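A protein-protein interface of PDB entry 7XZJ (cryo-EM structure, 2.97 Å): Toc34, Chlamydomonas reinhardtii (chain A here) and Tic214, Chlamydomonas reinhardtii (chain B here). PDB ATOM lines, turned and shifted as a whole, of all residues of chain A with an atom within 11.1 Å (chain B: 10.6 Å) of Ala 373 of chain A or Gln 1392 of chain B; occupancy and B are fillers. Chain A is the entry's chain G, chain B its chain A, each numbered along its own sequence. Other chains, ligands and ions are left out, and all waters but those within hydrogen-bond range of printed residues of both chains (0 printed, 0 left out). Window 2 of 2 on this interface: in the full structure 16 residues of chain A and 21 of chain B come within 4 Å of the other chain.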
ATOM      1  N   ALA A 365     -19.646  -6.201  13.904  1.00  0.00           N
ATOM      2  CA  ALA A 365     -19.632  -5.398  15.151  1.00  0.00           C
ATOM      3  C   ALA A 365     -18.458  -4.414  15.143  1.00  0.00           C
ATOM      4  O   ALA A 365     -18.659  -3.265  15.570  1.00  0.00           O
ATOM      5  CB  ALA A 365     -19.582  -6.308  16.353  1.00  0.00           C
ATOM      6  N   LEU A 366     -17.281  -4.853  14.686  1.00  0.00           N
ATOM      7  CA  LEU A 366     -16.096  -3.958  14.601  1.00  0.00           C
ATOM      8  C   LEU A 366     -16.391  -2.847  13.589  1.00  0.00           C
ATOM      9  O   LEU A 366     -16.011  -1.693  13.854  1.00  0.00           O
ATOM     10  CB  LEU A 366     -14.895  -4.795  14.149  1.00  0.00           C
ATOM     11  CG  LEU A 366     -13.588  -4.033  13.929  1.00  0.00           C
ATOM     12  CD1 LEU A 366     -13.108  -3.413  15.232  1.00  0.00           C
ATOM     13  CD2 LEU A 366     -12.515  -4.939  13.343  1.00  0.00           C
ATOM     14  N   ARG A 367     -17.041  -3.190  12.473  1.00  0.00           N
ATOM     15  CA  ARG A 367     -17.421  -2.176  11.452  1.00  0.00           C
ATOM     16  C   ARG A 367     -18.431  -1.217  12.089  1.00  0.00           C
ATOM     17  O   ARG A 367     -18.343  -0.008  11.822  1.00  0.00           O
ATOM     18  CB  ARG A 367     -17.982  -2.858  10.202  1.00  0.00           C
ATOM     19  CG  ARG A 367     -17.981  -1.984   8.957  1.00  0.00           C
ATOM     20  CD  ARG A 367     -17.970  -2.831   7.700  1.00  0.00           C
ATOM     21  NE  ARG A 367     -18.148  -2.029   6.500  1.00  0.00           N
ATOM     22  CZ  ARG A 367     -19.320  -1.806   5.919  1.00  0.00           C
ATOM     23  NH1 ARG A 367     -20.419  -2.335   6.425  1.00  0.00           N
ATOM     24  NH2 ARG A 367     -19.389  -1.060   4.832  1.00  0.00           N
ATOM     25  N   GLY A 368     -19.364  -1.744  12.886  1.00  0.00           N
ATOM     26  CA  GLY A 368     -20.332  -0.881  13.590  1.00  0.00           C
ATOM     27  C   GLY A 368     -19.620   0.028  14.574  1.00  0.00           C
ATOM     28  O   GLY A 368     -19.972   1.220  14.627  1.00  0.00           O
ATOM     29  N   GLN A 369     -18.659  -0.513  15.329  1.00  0.00           N
ATOM     30  CA  GLN A 369     -17.877   0.308  16.249  1.00  0.00           C
ATOM     31  C   GLN A 369     -17.159   1.426  15.508  1.00  0.00           C
ATOM     32  O   GLN A 369     -17.155   2.578  15.957  1.00  0.00           O
ATOM     33  CB  GLN A 369     -16.869  -0.558  17.008  1.00  0.00           C
ATOM     34  CG  GLN A 369     -15.867   0.224  17.854  1.00  0.00           C
ATOM     35  CD  GLN A 369     -14.657   0.691  17.065  1.00  0.00           C
ATOM     36  OE1 GLN A 369     -14.371   0.178  15.983  1.00  0.00           O
ATOM     37  NE2 GLN A 369     -13.946   1.678  17.597  1.00  0.00           N
ATOM     38  N   GLN A 370     -16.538   1.104  14.373  1.00  0.00           N
ATOM     39  CA  GLN A 370     -15.837   2.133  13.611  1.00  0.00           C
ATOM     40  C   GLN A 370     -16.810   3.189  13.099  1.00  0.00           C
ATOM     41  O   GLN A 370     -16.475   4.378  13.041  1.00  0.00           O
ATOM     42  CB  GLN A 370     -15.052   1.501  12.460  1.00  0.00           C
ATOM     43  CG  GLN A 370     -15.694   1.619  11.089  1.00  0.00           C
ATOM     44  CD  GLN A 370     -14.945   0.839  10.035  1.00  0.00           C
ATOM     45  OE1 GLN A 370     -13.958   0.167  10.332  1.00  0.00           O
ATOM     46  NE2 GLN A 370     -15.408   0.922   8.795  1.00  0.00           N
ATOM     47  N   ARG A 371     -18.020   2.772  12.719  1.00  0.00           N
ATOM     48  CA  ARG A 371     -19.013   3.732  12.246  1.00  0.00           C
ATOM     49  C   ARG A 371     -19.532   4.607  13.382  1.00  0.00           C
ATOM     50  O   ARG A 371     -19.930   5.754  13.153  1.00  0.00           O
ATOM     51  CB  ARG A 371     -20.169   3.005  11.564  1.00  0.00           C
ATOM     52  CG  ARG A 371     -20.972   3.890  10.632  1.00  0.00           C
ATOM     53  CD  ARG A 371     -20.148   4.305   9.425  1.00  0.00           C
ATOM     54  NE  ARG A 371     -20.154   3.294   8.379  1.00  0.00           N
ATOM     55  CZ  ARG A 371     -20.957   3.319   7.321  1.00  0.00           C
ATOM     56  NH1 ARG A 371     -21.831   4.296   7.141  1.00  0.00           N
ATOM     57  NH2 ARG A 371     -20.878   2.343   6.424  1.00  0.00           N
ATOM     58  N   ARG A 372     -19.565   4.072  14.607  1.00  0.00           N
ATOM     59  CA  ARG A 372     -20.075   4.842  15.739  1.00  0.00           C
ATOM     60  C   ARG A 372     -19.247   6.100  15.973  1.00  0.00           C
ATOM     61  O   ARG A 372     -19.799   7.172  16.249  1.00  0.00           O
ATOM     62  CB  ARG A 372     -20.104   3.979  16.998  1.00  0.00           C
ATOM     63  N   ALA A 373     -17.926   5.993  15.874  1.00  0.00           N
ATOM     64  CA  ALA A 373     -17.094   7.184  15.865  1.00  0.00           C
ATOM     65  C   ALA A 373     -17.388   8.001  14.613  1.00  0.00           C
ATOM     66  O   ALA A 373     -17.812   7.466  13.585  1.00  0.00           O
ATOM     67  CB  ALA A 373     -15.614   6.816  15.930  1.00  0.00           C
ATOM     68  N   LEU A 374     -17.182   9.314  14.721  1.00  0.00           N
ATOM     69  CA  LEU A 374     -17.545  10.324  13.729  1.00  0.00           C
ATOM     70  C   LEU A 374     -19.047  10.561  13.678  1.00  0.00           C
ATOM     71  O   LEU A 374     -19.502  11.388  12.881  1.00  0.00           O
ATOM     72  CB  LEU A 374     -17.047   9.987  12.315  1.00  0.00           C
ATOM     73  CG  LEU A 374     -15.580   9.591  12.162  1.00  0.00           C
ATOM     74  CD1 LEU A 374     -15.353   8.902  10.827  1.00  0.00           C
ATOM     75  CD2 LEU A 374     -14.693  10.816  12.292  1.00  0.00           C
ATOM     76  N   GLY A 375     -19.832   9.873  14.499  1.00  0.00           N
ATOM     77  CA  GLY A 375     -21.268  10.105  14.544  1.00  0.00           C
ATOM     78  C   GLY A 375     -21.996   9.803  13.254  1.00  0.00           C
ATOM     79  O   GLY A 375     -22.864  10.582  12.839  1.00  0.00           O
ATOM     80  N   LEU A 376     -21.648   8.689  12.608  1.00  0.00           N
ATOM     81  CA  LEU A 376     -22.303   8.327  11.324  1.00  0.00           C
ATOM     82  C   LEU A 376     -23.346   7.231  11.574  1.00  0.00           C
ATOM     83  O   LEU A 376     -23.162   6.449  12.524  1.00  0.00           O
ATOM     84  CB  LEU A 376     -21.234   7.883  10.321  1.00  0.00           C
ATOM     85  CG  LEU A 376     -20.224   8.957   9.923  1.00  0.00           C
ATOM     86  CD1 LEU A 376     -19.139   8.376   9.031  1.00  0.00           C
ATOM     87  CD2 LEU A 376     -20.918  10.120   9.229  1.00  0.00           C
ATOM     88  N   HIS A 377     -24.397   7.183  10.749  1.00  0.00           N
ATOM     89  CA  HIS A 377     -25.469   6.164  10.915  1.00  0.00           C
ATOM     90  C   HIS A 377     -24.880   4.766  10.711  1.00  0.00           C
ATOM     91  O   HIS A 377     -24.052   4.610   9.793  1.00  0.00           O
ATOM     92  CB  HIS A 377     -26.627   6.427   9.942  1.00  0.00           C
ATOM     93  CG  HIS A 377     -27.515   7.560  10.331  1.00  0.00           C
ATOM     94  ND1 HIS A 377     -27.062   8.862  10.418  1.00  0.00           N
ATOM     95  CD2 HIS A 377     -28.830   7.596  10.639  1.00  0.00           C
ATOM     96  CE1 HIS A 377     -28.058   9.649  10.771  1.00  0.00           C
ATOM     97  NE2 HIS A 377     -29.154   8.896  10.914  1.00  0.00           N
ATOM     98  N   ARG A 378     -25.314   3.789  11.513  1.00  0.00           N
ATOM     99  CA  ARG A 378     -24.754   2.411  11.436  1.00  0.00           C
ATOM    100  C   ARG A 378     -24.920   1.835  10.017  1.00  0.00           C
ATOM    101  O   ARG A 378     -25.940   2.173   9.383  1.00  0.00           O
ATOM    102  CB  ARG A 378     -25.419   1.506  12.477  1.00  0.00           C
ATOM    103  N   PRO A 379     -24.016   0.972   9.474  1.00  0.00           N
ATOM    104  CA  PRO A 379     -24.241   0.402   8.141  1.00  0.00           C
ATOM    105  C   PRO A 379     -25.473  -0.489   8.101  1.00  0.00           C
ATOM    106  O   PRO A 379     -25.767  -1.223   9.047  1.00  0.00           O
ATOM    107  CB  PRO A 379     -22.961  -0.397   7.876  1.00  0.00           C
ATOM    108  CG  PRO A 379     -22.422  -0.703   9.234  1.00  0.00           C
ATOM    109  CD  PRO A 379     -22.765   0.486  10.079  1.00  0.00           C
ATOM    110  N   ASP B1380      -5.825  -7.977  13.727  1.00  0.00           N
ATOM    111  CA  ASP B1380      -7.192  -7.694  14.243  1.00  0.00           C
ATOM    112  C   ASP B1380      -7.430  -6.183  14.292  1.00  0.00           C
ATOM    113  O   ASP B1380      -6.422  -5.446  14.308  1.00  0.00           O
ATOM    114  CB  ASP B1380      -7.406  -8.336  15.615  1.00  0.00           C
ATOM    115  N   ASN B1381      -8.700  -5.754  14.269  1.00  0.00           N
ATOM    116  CA  ASN B1381      -9.079  -4.312  14.306  1.00  0.00           C
ATOM    117  C   ASN B1381      -9.014  -3.717  12.894  1.00  0.00           C
ATOM    118  O   ASN B1381      -9.240  -2.498  12.762  1.00  0.00           O
ATOM    119  CB  ASN B1381      -8.327  -3.495  15.364  1.00  0.00           C
ATOM    120  CG  ASN B1381      -8.626  -3.930  16.784  1.00  0.00           C
ATOM    121  OD1 ASN B1381      -7.853  -3.652  17.697  1.00  0.00           O
ATOM    122  ND2 ASN B1381      -9.741  -4.616  16.979  1.00  0.00           N
ATOM    123  N   LEU B1382      -8.776  -4.554  11.878  1.00  0.00           N
ATOM    124  CA  LEU B1382      -8.747  -4.072  10.469  1.00  0.00           C
ATOM    125  C   LEU B1382      -9.849  -4.770   9.664  1.00  0.00           C
ATOM    126  O   LEU B1382      -9.795  -6.008   9.549  1.00  0.00           O
ATOM    127  CB  LEU B1382      -7.368  -4.363   9.869  1.00  0.00           C
ATOM    128  CG  LEU B1382      -6.196  -3.629  10.519  1.00  0.00           C
ATOM    129  CD1 LEU B1382      -4.874  -4.087   9.923  1.00  0.00           C
ATOM    130  CD2 LEU B1382      -6.354  -2.124  10.375  1.00  0.00           C
ATOM    131  N   THR B1383     -10.800  -4.003   9.123  1.00  0.00           N
ATOM    132  CA  THR B1383     -11.925  -4.581   8.336  1.00  0.00           C
ATOM    133  C   THR B1383     -11.878  -4.032   6.906  1.00  0.00           C
ATOM    134  O   THR B1383     -11.717  -2.808   6.759  1.00  0.00           O
ATOM    135  CB  THR B1383     -13.269  -4.296   9.017  1.00  0.00           C
ATOM    136  OG1 THR B1383     -13.279  -4.979  10.271  1.00  0.00           O
ATOM    137  CG2 THR B1383     -14.459  -4.730   8.191  1.00  0.00           C
ATOM    138  N   ILE B1388      -8.899  -1.197   3.183  1.00  0.00           N
ATOM    139  CA  ILE B1388      -8.644  -1.540   4.612  1.00  0.00           C
ATOM    140  C   ILE B1388      -9.034  -0.318   5.448  1.00  0.00           C
ATOM    141  O   ILE B1388      -8.615   0.799   5.089  1.00  0.00           O
ATOM    142  CB  ILE B1388      -7.171  -1.944   4.825  1.00  0.00           C
ATOM    143  CG1 ILE B1388      -6.734  -3.025   3.833  1.00  0.00           C
ATOM    144  CG2 ILE B1388      -6.926  -2.370   6.264  1.00  0.00           C
ATOM    145  CD1 ILE B1388      -5.309  -3.488   4.017  1.00  0.00           C
ATOM    146  N   THR B1389      -9.802  -0.529   6.519  1.00  0.00           N
ATOM    147  CA  THR B1389     -10.243   0.597   7.384  1.00  0.00           C
ATOM    148  C   THR B1389      -9.797   0.324   8.820  1.00  0.00           C
ATOM    149  O   THR B1389      -9.685  -0.863   9.183  1.00  0.00           O
ATOM    150  CB  THR B1389     -11.763   0.803   7.332  1.00  0.00           C
ATOM    151  OG1 THR B1389     -12.392  -0.351   7.889  1.00  0.00           O
ATOM    152  CG2 THR B1389     -12.289   1.055   5.936  1.00  0.00           C
ATOM    153  N   THR B1390      -9.556   1.382   9.595  1.00  0.00           N
ATOM    154  CA  THR B1390      -9.144   1.226  10.981  1.00  0.00           C
ATOM    155  C   THR B1390     -10.322   1.470  11.917  1.00  0.00           C
ATOM    156  O   THR B1390     -11.431   1.810  11.496  1.00  0.00           O
ATOM    157  CB  THR B1390      -7.993   2.180  11.310  1.00  0.00           C
ATOM    158  OG1 THR B1390      -7.506   1.908  12.630  1.00  0.00           O
ATOM    159  CG2 THR B1390      -8.465   3.624  11.243  1.00  0.00           C
ATOM    160  N   LEU B1391     -10.063   1.278  13.213  1.00  0.00           N
ATOM    161  CA  LEU B1391     -11.106   1.455  14.219  1.00  0.00           C
ATOM    162  C   LEU B1391     -11.610   2.892  14.268  1.00  0.00           C
ATOM    163  O   LEU B1391     -12.783   3.126  14.578  1.00  0.00           O
ATOM    164  CB  LEU B1391     -10.585   1.030  15.593  1.00  0.00           C
ATOM    165  N   GLN B1392     -10.743   3.864  13.976  1.00  0.00           N
ATOM    166  CA  GLN B1392     -11.167   5.261  13.969  1.00  0.00           C
ATOM    167  C   GLN B1392     -12.192   5.533  12.878  1.00  0.00           C
ATOM    168  O   GLN B1392     -12.976   6.483  12.984  1.00  0.00           O
ATOM    169  CB  GLN B1392      -9.959   6.183  13.800  1.00  0.00           C
ATOM    170  CG  GLN B1392      -9.124   6.364  15.058  1.00  0.00           C
ATOM    171  CD  GLN B1392      -8.272   5.154  15.380  1.00  0.00           C
ATOM    172  OE1 GLN B1392      -8.047   4.293  14.531  1.00  0.00           O
ATOM    173  NE2 GLN B1392      -7.789   5.085  16.615  1.00  0.00           N
ATOM    174  N   GLY B1393     -12.205   4.716  11.832  1.00  0.00           N
ATOM    175  CA  GLY B1393     -13.091   4.917  10.706  1.00  0.00           C
ATOM    176  C   GLY B1393     -12.439   5.492   9.470  1.00  0.00           C
ATOM    177  O   GLY B1393     -13.141   5.734   8.482  1.00  0.00           O
ATOM    178  N   ALA B1394     -11.131   5.716   9.490  1.00  0.00           N
ATOM    179  CA  ALA B1394     -10.394   6.215   8.340  1.00  0.00           C
ATOM    180  C   ALA B1394      -9.641   5.078   7.662  1.00  0.00           C
ATOM    181  O   ALA B1394      -9.563   3.956   8.165  1.00  0.00           O
ATOM    182  CB  ALA B1394      -9.422   7.319   8.761  1.00  0.00           C
ATOM    183  N   PHE B1395      -9.080   5.385   6.497  1.00  0.00           N
ATOM    184  CA  PHE B1395      -8.278   4.413   5.776  1.00  0.00           C
ATOM    185  C   PHE B1395      -6.872   4.357   6.360  1.00  0.00           C
ATOM    186  O   PHE B1395      -6.339   5.357   6.850  1.00  0.00           O
ATOM    187  CB  PHE B1395      -8.222   4.752   4.288  1.00  0.00           C
ATOM    188  CG  PHE B1395      -9.564   4.725   3.612  1.00  0.00           C
ATOM    189  CD1 PHE B1395     -10.638   4.069   4.191  1.00  0.00           C
ATOM    190  CD2 PHE B1395      -9.752   5.354   2.394  1.00  0.00           C
ATOM    191  CE1 PHE B1395     -11.872   4.046   3.574  1.00  0.00           C
ATOM    192  CE2 PHE B1395     -10.985   5.331   1.770  1.00  0.00           C
ATOM    193  CZ  PHE B1395     -12.045   4.677   2.362  1.00  0.00           C
ATOM    194  N   ILE B1396      -6.272   3.168   6.307  1.00  0.00           N
ATOM    195  CA  ILE B1396      -4.991   2.953   6.962  1.00  0.00           C
ATOM    196  C   ILE B1396      -3.885   3.679   6.200  1.00  0.00           C
ATOM    197  O   ILE B1396      -3.967   3.896   4.984  1.00  0.00           O
ATOM    198  CB  ILE B1396      -4.702   1.445   7.082  1.00  0.00           C
ATOM    199  CG1 ILE B1396      -3.537   1.187   8.039  1.00  0.00           C
ATOM    200  CG2 ILE B1396      -4.427   0.840   5.716  1.00  0.00           C
ATOM    201  CD1 ILE B1396      -3.278  -0.277   8.297  1.00  0.00           C
ATOM    202  N   THR B1397      -2.845   4.072   6.930  1.00  0.00           N
ATOM    203  CA  THR B1397      -1.699   4.780   6.384  1.00  0.00           C
ATOM    204  C   THR B1397      -0.501   3.839   6.316  1.00  0.00           C
ATOM    205  O   THR B1397      -0.445   2.825   7.014  1.00  0.00           O
ATOM    206  CB  THR B1397      -1.353   6.004   7.240  1.00  0.00           C
ATOM    207  OG1 THR B1397      -2.562   6.594   7.735  1.00  0.00           O
ATOM    208  CG2 THR B1397      -0.601   7.042   6.419  1.00  0.00           C
ATOM    209  N   GLU B1400       1.035   3.671   9.518  1.00  0.00           N
ATOM    210  CA  GLU B1400       0.107   2.907  10.397  1.00  0.00           C
ATOM    211  C   GLU B1400       0.195   1.417  10.045  1.00  0.00           C
ATOM    212  O   GLU B1400       0.177   0.595  10.978  1.00  0.00           O
ATOM    213  CB  GLU B1400      -1.322   3.432  10.259  1.00  0.00           C
ATOM    214  N   SER B1404       1.328  -1.435  12.522  1.00  0.00           N
ATOM    215  CA  SER B1404       0.429  -2.591  12.777  1.00  0.00           C
ATOM    216  C   SER B1404       1.196  -3.900  12.564  1.00  0.00           C
ATOM    217  O   SER B1404       1.042  -4.811  13.395  1.00  0.00           O
ATOM    218  CB  SER B1404      -0.787  -2.524  11.894  1.00  0.00           C
ATOM    219  OG  SER B1404      -1.549  -1.358  12.171  1.00  0.00           O
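OE1 of Gln 370 of chain A lies within hydrogen-bond range of OG1 of Thr 1389 of chain B (2.9 Å). The backbone carbonyl oxygen (O) of Thr 1390 of chain B lies close to the side-chain amide oxygen (OE1) of Gln 370 of chain A, 3.2 Å away.
The backbone carbonyl oxygen of Thr 1383 of chain B sits at hydrogen-bond distance from the side-chain hydroxyl of Thr 1389 of chain B (2.8 Å). OE1 of Gln 1392 of chain B is in hydrogen-bond range of OG1 of Thr 1390 of chain B, 3.1 Å away. OE1 of Gln 369 of chain A lies close to O of Leu 366 of chain A (3.3 Å).
Among the printed residues, merely in contact across the chains: Leu 366 of chain A with Asn 1381 of chain B, Leu 366 of chain A with Thr 1383 of chain B, Gln 369 of chain A with Leu 1391 of chain B, Gln 370 of chain A with Leu 1391 of chain B and Ala 373 of chain A with Gln 1392 of chain B.
Printed residues of chain B within 4 Å of Gln 369 of chain A: Leu 1391 (3.5 Å). Of the printed residues of chain B, Gln 370 of chain A touches Thr 1389 (2.9 Å), Thr 1390 (3.2 Å) and Leu 1391 (3.4 Å). No residue of chain B comes within 4 Å of Arg 372 of chain A. Ala 373 of chain A touches just one residue of chain B: Gln 1392 (3.97 Å). No residue of chain B comes within 4 Å of Gly 375 of chain A. No residue of chain B comes within 4 Å of Leu 376 of chain A. Asp 1380 of chain B touches none of the printed residues of chain A. Of the printed residues of chain A, Asn 1381 of chain B touches Leu 366 (3.6 Å). Leu 1382 of chain B touches none of the printed residues of chain A. Printed residues of chain A within 4 Å of Thr 1383 of chain B: Leu 366. Of the printed residues of chain A, Thr 1389 of chain B touches Gln 370 (2.9 Å). Of chain A, only Gln 370 (3.2 Å) comes within 4 Å of Thr 1390 of chain B. Of the printed residues of chain A, Gln 1392 of chain B touches Ala 373 (3.97 Å). No residue of chain A comes within 4 Å of Gly 1393 of chain B. The nearest residue of chain B that does not touch Ala 373 of chain A is Leu 1391 of chain B (4.8 Å). The nearest printed residue of chain A that does not touch Gln 1392 of chain B is Leu 374 of chain A (4.02 Å).
Printed residues of chain A that touch a printed residue of chain B: Leu 366, Gln 369, Gln 370 and Ala 373. Hydrophobic or aromatic side chains of chain A that line the printed part of chain B: Leu 366 and Ala 373. Printed residues of chain B that touch a printed residue of chain A: Asn 1381, Thr 1383, Thr 1389, Thr 1390, Leu 1391 and Gln 1392. Hydrophobic or aromatic side chains of chain B within 4 Å of the printed part of chain A: Leu 1391. Among the printed residues, no Asp or Glu carboxylate lies within 4 Å of a Lys or Arg side-chain nitrogen of the other chain.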
